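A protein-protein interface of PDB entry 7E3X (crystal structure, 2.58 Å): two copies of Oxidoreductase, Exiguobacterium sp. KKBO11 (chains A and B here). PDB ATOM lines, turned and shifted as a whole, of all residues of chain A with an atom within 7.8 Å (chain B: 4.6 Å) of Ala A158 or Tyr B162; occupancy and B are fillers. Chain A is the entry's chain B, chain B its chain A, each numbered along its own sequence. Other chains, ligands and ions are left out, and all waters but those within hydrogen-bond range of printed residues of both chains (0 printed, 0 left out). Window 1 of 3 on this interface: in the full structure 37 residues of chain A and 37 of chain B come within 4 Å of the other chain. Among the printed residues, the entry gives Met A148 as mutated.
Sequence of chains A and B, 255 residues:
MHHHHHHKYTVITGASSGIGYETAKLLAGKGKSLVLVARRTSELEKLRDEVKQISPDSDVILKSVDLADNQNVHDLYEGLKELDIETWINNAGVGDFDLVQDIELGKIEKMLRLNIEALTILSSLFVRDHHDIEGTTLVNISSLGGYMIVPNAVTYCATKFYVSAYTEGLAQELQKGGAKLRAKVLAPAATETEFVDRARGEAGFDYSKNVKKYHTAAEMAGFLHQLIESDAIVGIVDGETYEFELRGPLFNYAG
The backbone carbonyl oxygen (O) of Ile B116 is in hydrogen-bond range of the side-chain hydroxyl (OG1) of Thr B120 (2.7 Å). The side-chain hydroxyl (OG1) of Thr B120 lies within hydrogen-bond range of the side-chain hydroxyl (OH) of Tyr B162 (2.8 Å). The side-chain hydroxyl of Thr A159 is in hydrogen-bond range of the side-chain amide nitrogen of Asn A115, at 3.0 Å. The backbone carbonyl oxygen (O) of Tyr A156 sits at hydrogen-bond distance from the side-chain hydroxyl (OG1) of Thr A159, at 2.6 Å.
Among the printed residues, pairs that only touch across the chains: Ala A158 with Tyr B162, Ile A149 with Ala B165, Val A154 with Tyr B166, Tyr A162 with Ala B158, Ala A165 with Phe B161, Phe A161 with Ala B165, Leu A112 with Tyr B162, Thr A155 with Tyr B166, Thr A155 with Tyr B162, Tyr A162 with Ile B116, Thr A159 with Tyr B162, Ile A116 with Tyr B162, Ala A158 with Tyr B166, Tyr A162 with Thr B159 and Ile A116 with Ile B116.
Of chain B, only Tyr B162 and Tyr B166 come within 4 Å of Ala A158. Of chain A, only Leu A112 (3.5 Å), Ile A116 (3.6 Å), Thr A155 (3.5 Å), Ala A158 (3.1 Å) and Thr A159 (3.6 Å) come within 4 Å of Tyr B162. Printed residues of chain B within 4 Å of Ile A116: Ile B116 and Tyr B162. Printed residues of chain A within 4 Å of Tyr B166: Val A154, Thr A155 and Ala A158. Printed residues of chain A within 4 Å of Ile B116: Ile A116 (3.9 Å) and Tyr A162 (3.6 Å). Of the printed residues of chain B, Ala A165 touches Phe B161 (3.4 Å). Of the printed residues of chain B, Ile A149 touches Ala B165. Cys A157 touches none of the printed residues of chain B. Gly A146 touches none of the printed residues of chain B. The nearest printed residue of chain A that does not touch Tyr B166 is Ile A149 (5.1 Å).
Printed residues of chain A that touch a printed residue of chain B: Leu A112, Ile A116, Ile A149, Val A154, Thr A155, Ala A158, Thr A159, Phe A161, Tyr A162 and Ala A165. Hydrophobic or aromatic side chains of chain A within 4 Å of the printed part of chain B: Leu A112, Ile A116, Ile A149, Val A154, Ala A158, Phe A161, Tyr A162 and Ala A165. Among the printed residues, 15 pairs touch across the chains. Among the printed residues, no Asp or Glu carboxylate lies within 4 Å of a Lys or Arg side-chain nitrogen of the other chain.
Ile B116 touches its own counterpart, Ile A116. Ala A158 touches Tyr B162, and with the chains exchanged Tyr A162 touches Ala B158. Thr A159 touches Tyr B162, and with the chains exchanged Tyr A162 touches Thr B159. Phe A161 touches Ala B165, and with the chains exchanged Ala A165 touches Phe B161. 9 positions are printed for both chains. Of the 15 pairs that touch across the chains among the printed residues, 9 have their exchanged pair printed and touching as well.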
ATOM      1  N   ILE A 108     -16.489  -4.394 -28.796  1.00  0.00           N
ATOM      2  CA  ILE A 108     -15.931  -3.403 -27.884  1.00  0.00           C
ATOM      3  C   ILE A 108     -17.043  -2.729 -27.105  1.00  0.00           C
ATOM      4  O   ILE A 108     -16.933  -2.527 -25.888  1.00  0.00           O
ATOM      5  CB  ILE A 108     -15.065  -2.385 -28.648  1.00  0.00           C
ATOM      6  CG1 ILE A 108     -13.589  -2.813 -28.614  1.00  0.00           C
ATOM      7  CG2 ILE A 108     -15.204  -1.001 -28.040  1.00  0.00           C
ATOM      8  CD1 ILE A 108     -13.320  -4.226 -29.142  1.00  0.00           C
ATOM      9  N   MET A 111     -18.099  -4.753 -24.424  1.00  0.00           N
ATOM     10  CA  MET A 111     -17.076  -4.731 -23.381  1.00  0.00           C
ATOM     11  C   MET A 111     -17.247  -3.522 -22.478  1.00  0.00           C
ATOM     12  O   MET A 111     -17.274  -3.651 -21.246  1.00  0.00           O
ATOM     13  CB  MET A 111     -15.682  -4.733 -23.999  1.00  0.00           C
ATOM     14  CG  MET A 111     -14.594  -5.067 -23.024  1.00  0.00           C
ATOM     15  SD  MET A 111     -12.990  -5.121 -23.822  1.00  0.00           S
ATOM     16  CE  MET A 111     -12.889  -3.528 -24.598  1.00  0.00           C
ATOM     17  N   LEU A 112     -17.375  -2.335 -23.074  1.00  0.00           N
ATOM     18  CA  LEU A 112     -17.612  -1.145 -22.269  1.00  0.00           C
ATOM     19  C   LEU A 112     -18.804  -1.350 -21.350  1.00  0.00           C
ATOM     20  O   LEU A 112     -18.744  -1.032 -20.154  1.00  0.00           O
ATOM     21  CB  LEU A 112     -17.824   0.076 -23.163  1.00  0.00           C
ATOM     22  CG  LEU A 112     -16.696   0.386 -24.135  1.00  0.00           C
ATOM     23  CD1 LEU A 112     -16.972   1.662 -24.888  1.00  0.00           C
ATOM     24  CD2 LEU A 112     -15.387   0.491 -23.387  1.00  0.00           C
ATOM     25  N   ASN A 115     -17.740  -4.200 -18.651  1.00  0.00           N
ATOM     26  CA  ASN A 115     -16.577  -3.897 -17.828  1.00  0.00           C
ATOM     27  C   ASN A 115     -16.750  -2.618 -17.022  1.00  0.00           C
ATOM     28  O   ASN A 115     -16.264  -2.525 -15.888  1.00  0.00           O
ATOM     29  CB  ASN A 115     -15.348  -3.769 -18.712  1.00  0.00           C
ATOM     30  CG  ASN A 115     -14.914  -5.075 -19.262  1.00  0.00           C
ATOM     31  OD1 ASN A 115     -15.703  -6.017 -19.343  1.00  0.00           O
ATOM     32  ND2 ASN A 115     -13.630  -5.179 -19.584  1.00  0.00           N
ATOM     33  N   ILE A 116     -17.399  -1.611 -17.594  1.00  0.00           N
ATOM     34  CA  ILE A 116     -17.508  -0.293 -16.979  1.00  0.00           C
ATOM     35  C   ILE A 116     -18.913  -0.057 -16.439  1.00  0.00           C
ATOM     36  O   ILE A 116     -19.100   0.125 -15.239  1.00  0.00           O
ATOM     37  CB  ILE A 116     -17.094   0.812 -17.974  1.00  0.00           C
ATOM     38  CG1 ILE A 116     -15.664   0.572 -18.462  1.00  0.00           C
ATOM     39  CG2 ILE A 116     -17.177   2.164 -17.323  1.00  0.00           C
ATOM     40  CD1 ILE A 116     -15.208   1.527 -19.574  1.00  0.00           C
ATOM     41  N   GLY A 145      -3.472  -4.821 -15.921  1.00  0.00           N
ATOM     42  CA  GLY A 145      -3.673  -4.022 -17.110  1.00  0.00           C
ATOM     43  C   GLY A 145      -4.465  -2.767 -16.856  1.00  0.00           C
ATOM     44  O   GLY A 145      -4.528  -1.908 -17.741  1.00  0.00           O
ATOM     45  N   GLY A 146      -5.065  -2.635 -15.673  1.00  0.00           N
ATOM     46  CA  GLY A 146      -5.637  -1.377 -15.230  1.00  0.00           C
ATOM     47  C   GLY A 146      -4.665  -0.407 -14.577  1.00  0.00           C
ATOM     48  O   GLY A 146      -5.066   0.692 -14.169  1.00  0.00           O
ATOM     49  N   MET A 148      -1.239  -0.520 -15.985  1.00  0.00           N
ATOM     50  CA  MET A 148      -0.116  -0.610 -16.903  1.00  0.00           C
ATOM     51  C   MET A 148      -0.697  -1.029 -18.248  1.00  0.00           C
ATOM     52  O   MET A 148      -1.212  -2.142 -18.368  1.00  0.00           O
ATOM     53  CB  MET A 148       0.889  -1.613 -16.377  1.00  0.00           C
ATOM     54  CG  MET A 148       2.149  -1.765 -17.177  1.00  0.00           C
ATOM     55  SD  MET A 148       2.910  -3.342 -16.723  1.00  0.00           S
ATOM     56  CE  MET A 148       1.492  -4.419 -16.860  1.00  0.00           C
ATOM     57  N   ILE A 149      -0.645  -0.131 -19.235  1.00  0.00           N
ATOM     58  CA  ILE A 149      -1.204  -0.408 -20.554  1.00  0.00           C
ATOM     59  C   ILE A 149      -0.391  -1.495 -21.240  1.00  0.00           C
ATOM     60  O   ILE A 149       0.845  -1.430 -21.284  1.00  0.00           O
ATOM     61  CB  ILE A 149      -1.229   0.862 -21.413  1.00  0.00           C
ATOM     62  CG1 ILE A 149      -2.146   1.915 -20.775  1.00  0.00           C
ATOM     63  CG2 ILE A 149      -1.656   0.511 -22.840  1.00  0.00           C
ATOM     64  CD1 ILE A 149      -2.094   3.275 -21.429  1.00  0.00           C
ATOM     65  N   VAL A 150      -1.085  -2.484 -21.785  1.00  0.00           N
ATOM     66  CA  VAL A 150      -0.488  -3.632 -22.463  1.00  0.00           C
ATOM     67  C   VAL A 150      -0.710  -3.473 -23.959  1.00  0.00           C
ATOM     68  O   VAL A 150      -1.861  -3.312 -24.389  1.00  0.00           O
ATOM     69  CB  VAL A 150      -1.118  -4.951 -21.990  1.00  0.00           C
ATOM     70  CG1 VAL A 150      -0.563  -6.098 -22.804  1.00  0.00           C
ATOM     71  CG2 VAL A 150      -0.929  -5.140 -20.503  1.00  0.00           C
ATOM     72  N   ALA A 153      -3.988  -4.523 -26.317  1.00  0.00           N
ATOM     73  CA  ALA A 153      -5.198  -4.593 -25.496  1.00  0.00           C
ATOM     74  C   ALA A 153      -5.523  -3.203 -24.952  1.00  0.00           C
ATOM     75  O   ALA A 153      -5.838  -3.017 -23.778  1.00  0.00           O
ATOM     76  CB  ALA A 153      -5.050  -5.631 -24.382  1.00  0.00           C
ATOM     77  N   VAL A 154      -5.462  -2.203 -25.833  1.00  0.00           N
ATOM     78  CA  VAL A 154      -5.614  -0.812 -25.409  1.00  0.00           C
ATOM     79  C   VAL A 154      -7.013  -0.557 -24.863  1.00  0.00           C
ATOM     80  O   VAL A 154      -7.178   0.032 -23.793  1.00  0.00           O
ATOM     81  CB  VAL A 154      -5.276   0.134 -26.575  1.00  0.00           C
ATOM     82  CG1 VAL A 154      -5.656   1.547 -26.236  1.00  0.00           C
ATOM     83  CG2 VAL A 154      -3.799   0.039 -26.897  1.00  0.00           C
ATOM     84  N   THR A 155      -8.045  -0.983 -25.594  1.00  0.00           N
ATOM     85  CA  THR A 155      -9.410  -0.701 -25.158  1.00  0.00           C
ATOM     86  C   THR A 155      -9.749  -1.458 -23.881  1.00  0.00           C
ATOM     87  O   THR A 155     -10.384  -0.903 -22.974  1.00  0.00           O
ATOM     88  CB  THR A 155     -10.405  -1.038 -26.270  1.00  0.00           C
ATOM     89  OG1 THR A 155      -9.974  -0.453 -27.517  1.00  0.00           O
ATOM     90  CG2 THR A 155     -11.783  -0.502 -25.920  1.00  0.00           C
ATOM     91  N   TYR A 156      -9.343  -2.728 -23.790  1.00  0.00           N
ATOM     92  CA  TYR A 156      -9.551  -3.472 -22.554  1.00  0.00           C
ATOM     93  C   TYR A 156      -8.849  -2.786 -21.379  1.00  0.00           C
ATOM     94  O   TYR A 156      -9.501  -2.401 -20.398  1.00  0.00           O
ATOM     95  CB  TYR A 156      -9.085  -4.915 -22.726  1.00  0.00           C
ATOM     96  CG  TYR A 156      -8.975  -5.691 -21.441  1.00  0.00           C
ATOM     97  CD1 TYR A 156     -10.108  -6.164 -20.799  1.00  0.00           C
ATOM     98  CD2 TYR A 156      -7.746  -5.936 -20.861  1.00  0.00           C
ATOM     99  CE1 TYR A 156     -10.019  -6.865 -19.611  1.00  0.00           C
ATOM    100  CE2 TYR A 156      -7.645  -6.654 -19.660  1.00  0.00           C
ATOM    101  CZ  TYR A 156      -8.789  -7.110 -19.039  1.00  0.00           C
ATOM    102  OH  TYR A 156      -8.696  -7.825 -17.855  1.00  0.00           O
ATOM    103  N   CYS A 157      -7.523  -2.586 -21.473  1.00  0.00           N
ATOM    104  CA  CYS A 157      -6.785  -1.884 -20.417  1.00  0.00           C
ATOM    105  C   CYS A 157      -7.461  -0.602 -19.973  1.00  0.00           C
ATOM    106  O   CYS A 157      -7.509  -0.289 -18.769  1.00  0.00           O
ATOM    107  CB  CYS A 157      -5.378  -1.581 -20.887  1.00  0.00           C
ATOM    108  SG  CYS A 157      -4.396  -3.057 -20.954  1.00  0.00           S
ATOM    109  N   ALA A 158      -7.973   0.159 -20.930  1.00  0.00           N
ATOM    110  CA  ALA A 158      -8.666   1.383 -20.574  1.00  0.00           C
ATOM    111  C   ALA A 158      -9.914   1.105 -19.731  1.00  0.00           C
ATOM    112  O   ALA A 158     -10.237   1.894 -18.827  1.00  0.00           O
ATOM    113  CB  ALA A 158      -9.016   2.168 -21.830  1.00  0.00           C
ATOM    114  N   THR A 159     -10.642   0.007 -20.002  1.00  0.00           N
ATOM    115  CA  THR A 159     -11.755  -0.306 -19.106  1.00  0.00           C
ATOM    116  C   THR A 159     -11.248  -0.716 -17.729  1.00  0.00           C
ATOM    117  O   THR A 159     -11.931  -0.491 -16.725  1.00  0.00           O
ATOM    118  CB  THR A 159     -12.674  -1.409 -19.664  1.00  0.00           C
ATOM    119  OG1 THR A 159     -12.019  -2.679 -19.631  1.00  0.00           O
ATOM    120  CG2 THR A 159     -13.123  -1.100 -21.063  1.00  0.00           C
ATOM    121  N   LYS A 160     -10.047  -1.274 -17.653  1.00  0.00           N
ATOM    122  CA  LYS A 160      -9.544  -1.658 -16.346  1.00  0.00           C
ATOM    123  C   LYS A 160      -8.931  -0.479 -15.598  1.00  0.00           C
ATOM    124  O   LYS A 160      -9.041  -0.419 -14.367  1.00  0.00           O
ATOM    125  CB  LYS A 160      -8.553  -2.812 -16.483  1.00  0.00           C
ATOM    126  CG  LYS A 160      -9.213  -4.130 -16.898  1.00  0.00           C
ATOM    127  CD  LYS A 160     -10.533  -4.318 -16.180  1.00  0.00           C
ATOM    128  CE  LYS A 160     -11.025  -5.746 -16.300  1.00  0.00           C
ATOM    129  NZ  LYS A 160     -12.149  -6.050 -15.361  1.00  0.00           N
ATOM    130  N   PHE A 161      -8.322   0.477 -16.309  1.00  0.00           N
ATOM    131  CA  PHE A 161      -7.949   1.740 -15.673  1.00  0.00           C
ATOM    132  C   PHE A 161      -9.171   2.443 -15.094  1.00  0.00           C
ATOM    133  O   PHE A 161      -9.085   3.087 -14.035  1.00  0.00           O
ATOM    134  CB  PHE A 161      -7.263   2.667 -16.673  1.00  0.00           C
ATOM    135  CG  PHE A 161      -5.785   2.531 -16.722  1.00  0.00           C
ATOM    136  CD1 PHE A 161      -5.197   1.458 -17.365  1.00  0.00           C
ATOM    137  CD2 PHE A 161      -4.975   3.495 -16.155  1.00  0.00           C
ATOM    138  CE1 PHE A 161      -3.818   1.340 -17.423  1.00  0.00           C
ATOM    139  CE2 PHE A 161      -3.591   3.386 -16.205  1.00  0.00           C
ATOM    140  CZ  PHE A 161      -3.008   2.312 -16.845  1.00  0.00           C
ATOM    141  N   TYR A 162     -10.311   2.366 -15.794  1.00  0.00           N
ATOM    142  CA  TYR A 162     -11.545   2.923 -15.247  1.00  0.00           C
ATOM    143  C   TYR A 162     -11.917   2.218 -13.953  1.00  0.00           C
ATOM    144  O   TYR A 162     -12.322   2.853 -12.977  1.00  0.00           O
ATOM    145  CB  TYR A 162     -12.701   2.811 -16.255  1.00  0.00           C
ATOM    146  CG  TYR A 162     -14.038   3.211 -15.638  1.00  0.00           C
ATOM    147  CD1 TYR A 162     -14.719   2.355 -14.764  1.00  0.00           C
ATOM    148  CD2 TYR A 162     -14.596   4.467 -15.893  1.00  0.00           C
ATOM    149  CE1 TYR A 162     -15.890   2.738 -14.164  1.00  0.00           C
ATOM    150  CE2 TYR A 162     -15.787   4.849 -15.307  1.00  0.00           C
ATOM    151  CZ  TYR A 162     -16.429   3.978 -14.447  1.00  0.00           C
ATOM    152  OH  TYR A 162     -17.613   4.344 -13.857  1.00  0.00           O
ATOM    153  N   VAL A 163     -11.848   0.893 -13.943  1.00  0.00           N
ATOM    154  CA  VAL A 163     -12.247   0.178 -12.741  1.00  0.00           C
ATOM    155  C   VAL A 163     -11.280   0.479 -11.609  1.00  0.00           C
ATOM    156  O   VAL A 163     -11.692   0.663 -10.461  1.00  0.00           O
ATOM    157  CB  VAL A 163     -12.357  -1.330 -13.019  1.00  0.00           C
ATOM    158  CG1 VAL A 163     -12.580  -2.055 -11.733  1.00  0.00           C
ATOM    159  CG2 VAL A 163     -13.506  -1.614 -14.009  1.00  0.00           C
ATOM    160  N   SER A 164      -9.988   0.560 -11.920  1.00  0.00           N
ATOM    161  CA  SER A 164      -8.999   0.875 -10.903  1.00  0.00           C
ATOM    162  C   SER A 164      -9.249   2.260 -10.328  1.00  0.00           C
ATOM    163  O   SER A 164      -9.377   2.431  -9.115  1.00  0.00           O
ATOM    164  CB  SER A 164      -7.605   0.784 -11.513  1.00  0.00           C
ATOM    165  OG  SER A 164      -7.189  -0.564 -11.596  1.00  0.00           O
ATOM    166  N   ALA A 165      -9.347   3.271 -11.194  1.00  0.00           N
ATOM    167  CA  ALA A 165      -9.537   4.631 -10.700  1.00  0.00           C
ATOM    168  C   ALA A 165     -10.900   4.795 -10.051  1.00  0.00           C
ATOM    169  O   ALA A 165     -11.033   5.517  -9.050  1.00  0.00           O
ATOM    170  CB  ALA A 165      -9.356   5.646 -11.831  1.00  0.00           C
ATOM    171  N   ILE B 116     -17.115   8.095 -22.288  1.00  0.00           N
ATOM    172  CA  ILE B 116     -16.327   6.913 -22.621  1.00  0.00           C
ATOM    173  C   ILE B 116     -16.752   6.300 -23.952  1.00  0.00           C
ATOM    174  O   ILE B 116     -15.922   6.058 -24.827  1.00  0.00           O
ATOM    175  CB  ILE B 116     -16.389   5.860 -21.497  1.00  0.00           C
ATOM    176  CG1 ILE B 116     -15.821   6.431 -20.206  1.00  0.00           C
ATOM    177  CG2 ILE B 116     -15.648   4.596 -21.950  1.00  0.00           C
ATOM    178  CD1 ILE B 116     -15.979   5.516 -19.053  1.00  0.00           C
ATOM    179  N   THR B 120     -14.945   6.496 -27.538  1.00  0.00           N
ATOM    180  CA  THR B 120     -14.299   5.281 -28.010  1.00  0.00           C
ATOM    181  C   THR B 120     -14.806   4.903 -29.393  1.00  0.00           C
ATOM    182  O   THR B 120     -14.008   4.575 -30.282  1.00  0.00           O
ATOM    183  CB  THR B 120     -14.524   4.148 -27.010  1.00  0.00           C
ATOM    184  OG1 THR B 120     -13.910   4.483 -25.758  1.00  0.00           O
ATOM    185  CG2 THR B 120     -13.919   2.858 -27.514  1.00  0.00           C
ATOM    186  N   ALA B 158     -12.917   8.701 -13.059  1.00  0.00           N
ATOM    187  CA  ALA B 158     -12.818   7.388 -13.653  1.00  0.00           C
ATOM    188  C   ALA B 158     -12.992   7.462 -15.161  1.00  0.00           C
ATOM    189  O   ALA B 158     -12.203   6.869 -15.901  1.00  0.00           O
ATOM    190  CB  ALA B 158     -13.836   6.452 -13.019  1.00  0.00           C
ATOM    191  N   THR B 159     -13.992   8.214 -15.650  1.00  0.00           N
ATOM    192  CA  THR B 159     -14.144   8.280 -17.103  1.00  0.00           C
ATOM    193  C   THR B 159     -12.966   8.988 -17.754  1.00  0.00           C
ATOM    194  O   THR B 159     -12.606   8.662 -18.885  1.00  0.00           O
ATOM    195  CB  THR B 159     -15.449   8.968 -17.543  1.00  0.00           C
ATOM    196  OG1 THR B 159     -15.358  10.391 -17.369  1.00  0.00           O
ATOM    197  CG2 THR B 159     -16.665   8.406 -16.815  1.00  0.00           C
ATOM    198  N   LYS B 160     -12.339   9.937 -17.066  1.00  0.00           N
ATOM    199  CA  LYS B 160     -11.188  10.598 -17.673  1.00  0.00           C
ATOM    200  C   LYS B 160      -9.934   9.741 -17.577  1.00  0.00           C
ATOM    201  O   LYS B 160      -9.057   9.839 -18.444  1.00  0.00           O
ATOM    202  CB  LYS B 160     -10.945  11.957 -17.020  1.00  0.00           C
ATOM    203  CG  LYS B 160     -12.019  12.967 -17.303  1.00  0.00           C
ATOM    204  CD  LYS B 160     -12.323  13.006 -18.777  1.00  0.00           C
ATOM    205  CE  LYS B 160     -13.344  14.093 -19.110  1.00  0.00           C
ATOM    206  NZ  LYS B 160     -13.276  14.488 -20.555  1.00  0.00           N
ATOM    207  N   PHE B 161      -9.816   8.923 -16.520  1.00  0.00           N
ATOM    208  CA  PHE B 161      -8.743   7.942 -16.485  1.00  0.00           C
ATOM    209  C   PHE B 161      -8.841   7.016 -17.683  1.00  0.00           C
ATOM    210  O   PHE B 161      -7.831   6.743 -18.342  1.00  0.00           O
ATOM    211  CB  PHE B 161      -8.791   7.161 -15.179  1.00  0.00           C
ATOM    212  CG  PHE B 161      -7.891   7.725 -14.089  1.00  0.00           C
ATOM    213  CD1 PHE B 161      -8.244   8.879 -13.402  1.00  0.00           C
ATOM    214  CD2 PHE B 161      -6.696   7.094 -13.756  1.00  0.00           C
ATOM    215  CE1 PHE B 161      -7.435   9.395 -12.413  1.00  0.00           C
ATOM    216  CE2 PHE B 161      -5.872   7.609 -12.764  1.00  0.00           C
ATOM    217  CZ  PHE B 161      -6.240   8.760 -12.087  1.00  0.00           C
ATOM    218  N   TYR B 162     -10.065   6.567 -18.012  1.00  0.00           N
ATOM    219  CA  TYR B 162     -10.289   5.787 -19.230  1.00  0.00           C
ATOM    220  C   TYR B 162      -9.801   6.536 -20.461  1.00  0.00           C
ATOM    221  O   TYR B 162      -9.131   5.959 -21.322  1.00  0.00           O
ATOM    222  CB  TYR B 162     -11.778   5.435 -19.411  1.00  0.00           C
ATOM    223  CG  TYR B 162     -12.037   4.653 -20.707  1.00  0.00           C
ATOM    224  CD1 TYR B 162     -12.040   5.285 -21.954  1.00  0.00           C
ATOM    225  CD2 TYR B 162     -12.232   3.274 -20.683  1.00  0.00           C
ATOM    226  CE1 TYR B 162     -12.228   4.572 -23.119  1.00  0.00           C
ATOM    227  CE2 TYR B 162     -12.441   2.552 -21.849  1.00  0.00           C
ATOM    228  CZ  TYR B 162     -12.436   3.204 -23.062  1.00  0.00           C
ATOM    229  OH  TYR B 162     -12.638   2.498 -24.231  1.00  0.00           O
ATOM    230  N   VAL B 163     -10.204   7.799 -20.603  1.00  0.00           N
ATOM    231  CA  VAL B 163      -9.805   8.557 -21.779  1.00  0.00           C
ATOM    232  C   VAL B 163      -8.290   8.699 -21.832  1.00  0.00           C
ATOM    233  O   VAL B 163      -7.681   8.590 -22.902  1.00  0.00           O
ATOM    234  CB  VAL B 163     -10.514   9.919 -21.790  1.00  0.00           C
ATOM    235  CG1 VAL B 163      -9.889  10.827 -22.827  1.00  0.00           C
ATOM    236  CG2 VAL B 163     -11.996   9.720 -22.064  1.00  0.00           C
ATOM    237  N   SER B 164      -7.655   8.903 -20.675  1.00  0.00           N
ATOM    238  CA  SER B 164      -6.203   9.041 -20.651  1.00  0.00           C
ATOM    239  C   SER B 164      -5.527   7.739 -21.064  1.00  0.00           C
ATOM    240  O   SER B 164      -4.682   7.726 -21.970  1.00  0.00           O
ATOM    241  CB  SER B 164      -5.731   9.484 -19.267  1.00  0.00           C
ATOM    242  OG  SER B 164      -6.164  10.804 -18.981  1.00  0.00           O
ATOM    243  N   ALA B 165      -5.889   6.630 -20.421  1.00  0.00           N
ATOM    244  CA  ALA B 165      -5.214   5.372 -20.718  1.00  0.00           C
ATOM    245  C   ALA B 165      -5.501   4.925 -22.143  1.00  0.00           C
ATOM    246  O   ALA B 165      -4.610   4.418 -22.831  1.00  0.00           O
ATOM    247  CB  ALA B 165      -5.636   4.299 -19.716  1.00  0.00           C
ATOM    248  N   TYR B 166      -6.736   5.115 -22.603  1.00  0.00           N
ATOM    249  CA  TYR B 166      -7.097   4.714 -23.956  1.00  0.00           C
ATOM    250  C   TYR B 166      -6.257   5.449 -24.988  1.00  0.00           C
ATOM    251  O   TYR B 166      -5.716   4.836 -25.920  1.00  0.00           O
ATOM    252  CB  TYR B 166      -8.580   4.985 -24.209  1.00  0.00           C
ATOM    253  CG  TYR B 166      -9.031   4.667 -25.624  1.00  0.00           C
ATOM    254  CD1 TYR B 166      -9.356   3.374 -25.986  1.00  0.00           C
ATOM    255  CD2 TYR B 166      -9.118   5.662 -26.592  1.00  0.00           C
ATOM    256  CE1 TYR B 166      -9.763   3.075 -27.263  1.00  0.00           C
ATOM    257  CE2 TYR B 166      -9.515   5.374 -27.874  1.00  0.00           C
ATOM    258  CZ  TYR B 166      -9.846   4.070 -28.208  1.00  0.00           C
ATOM    259  OH  TYR B 166     -10.256   3.757 -29.491  1.00  0.00           O
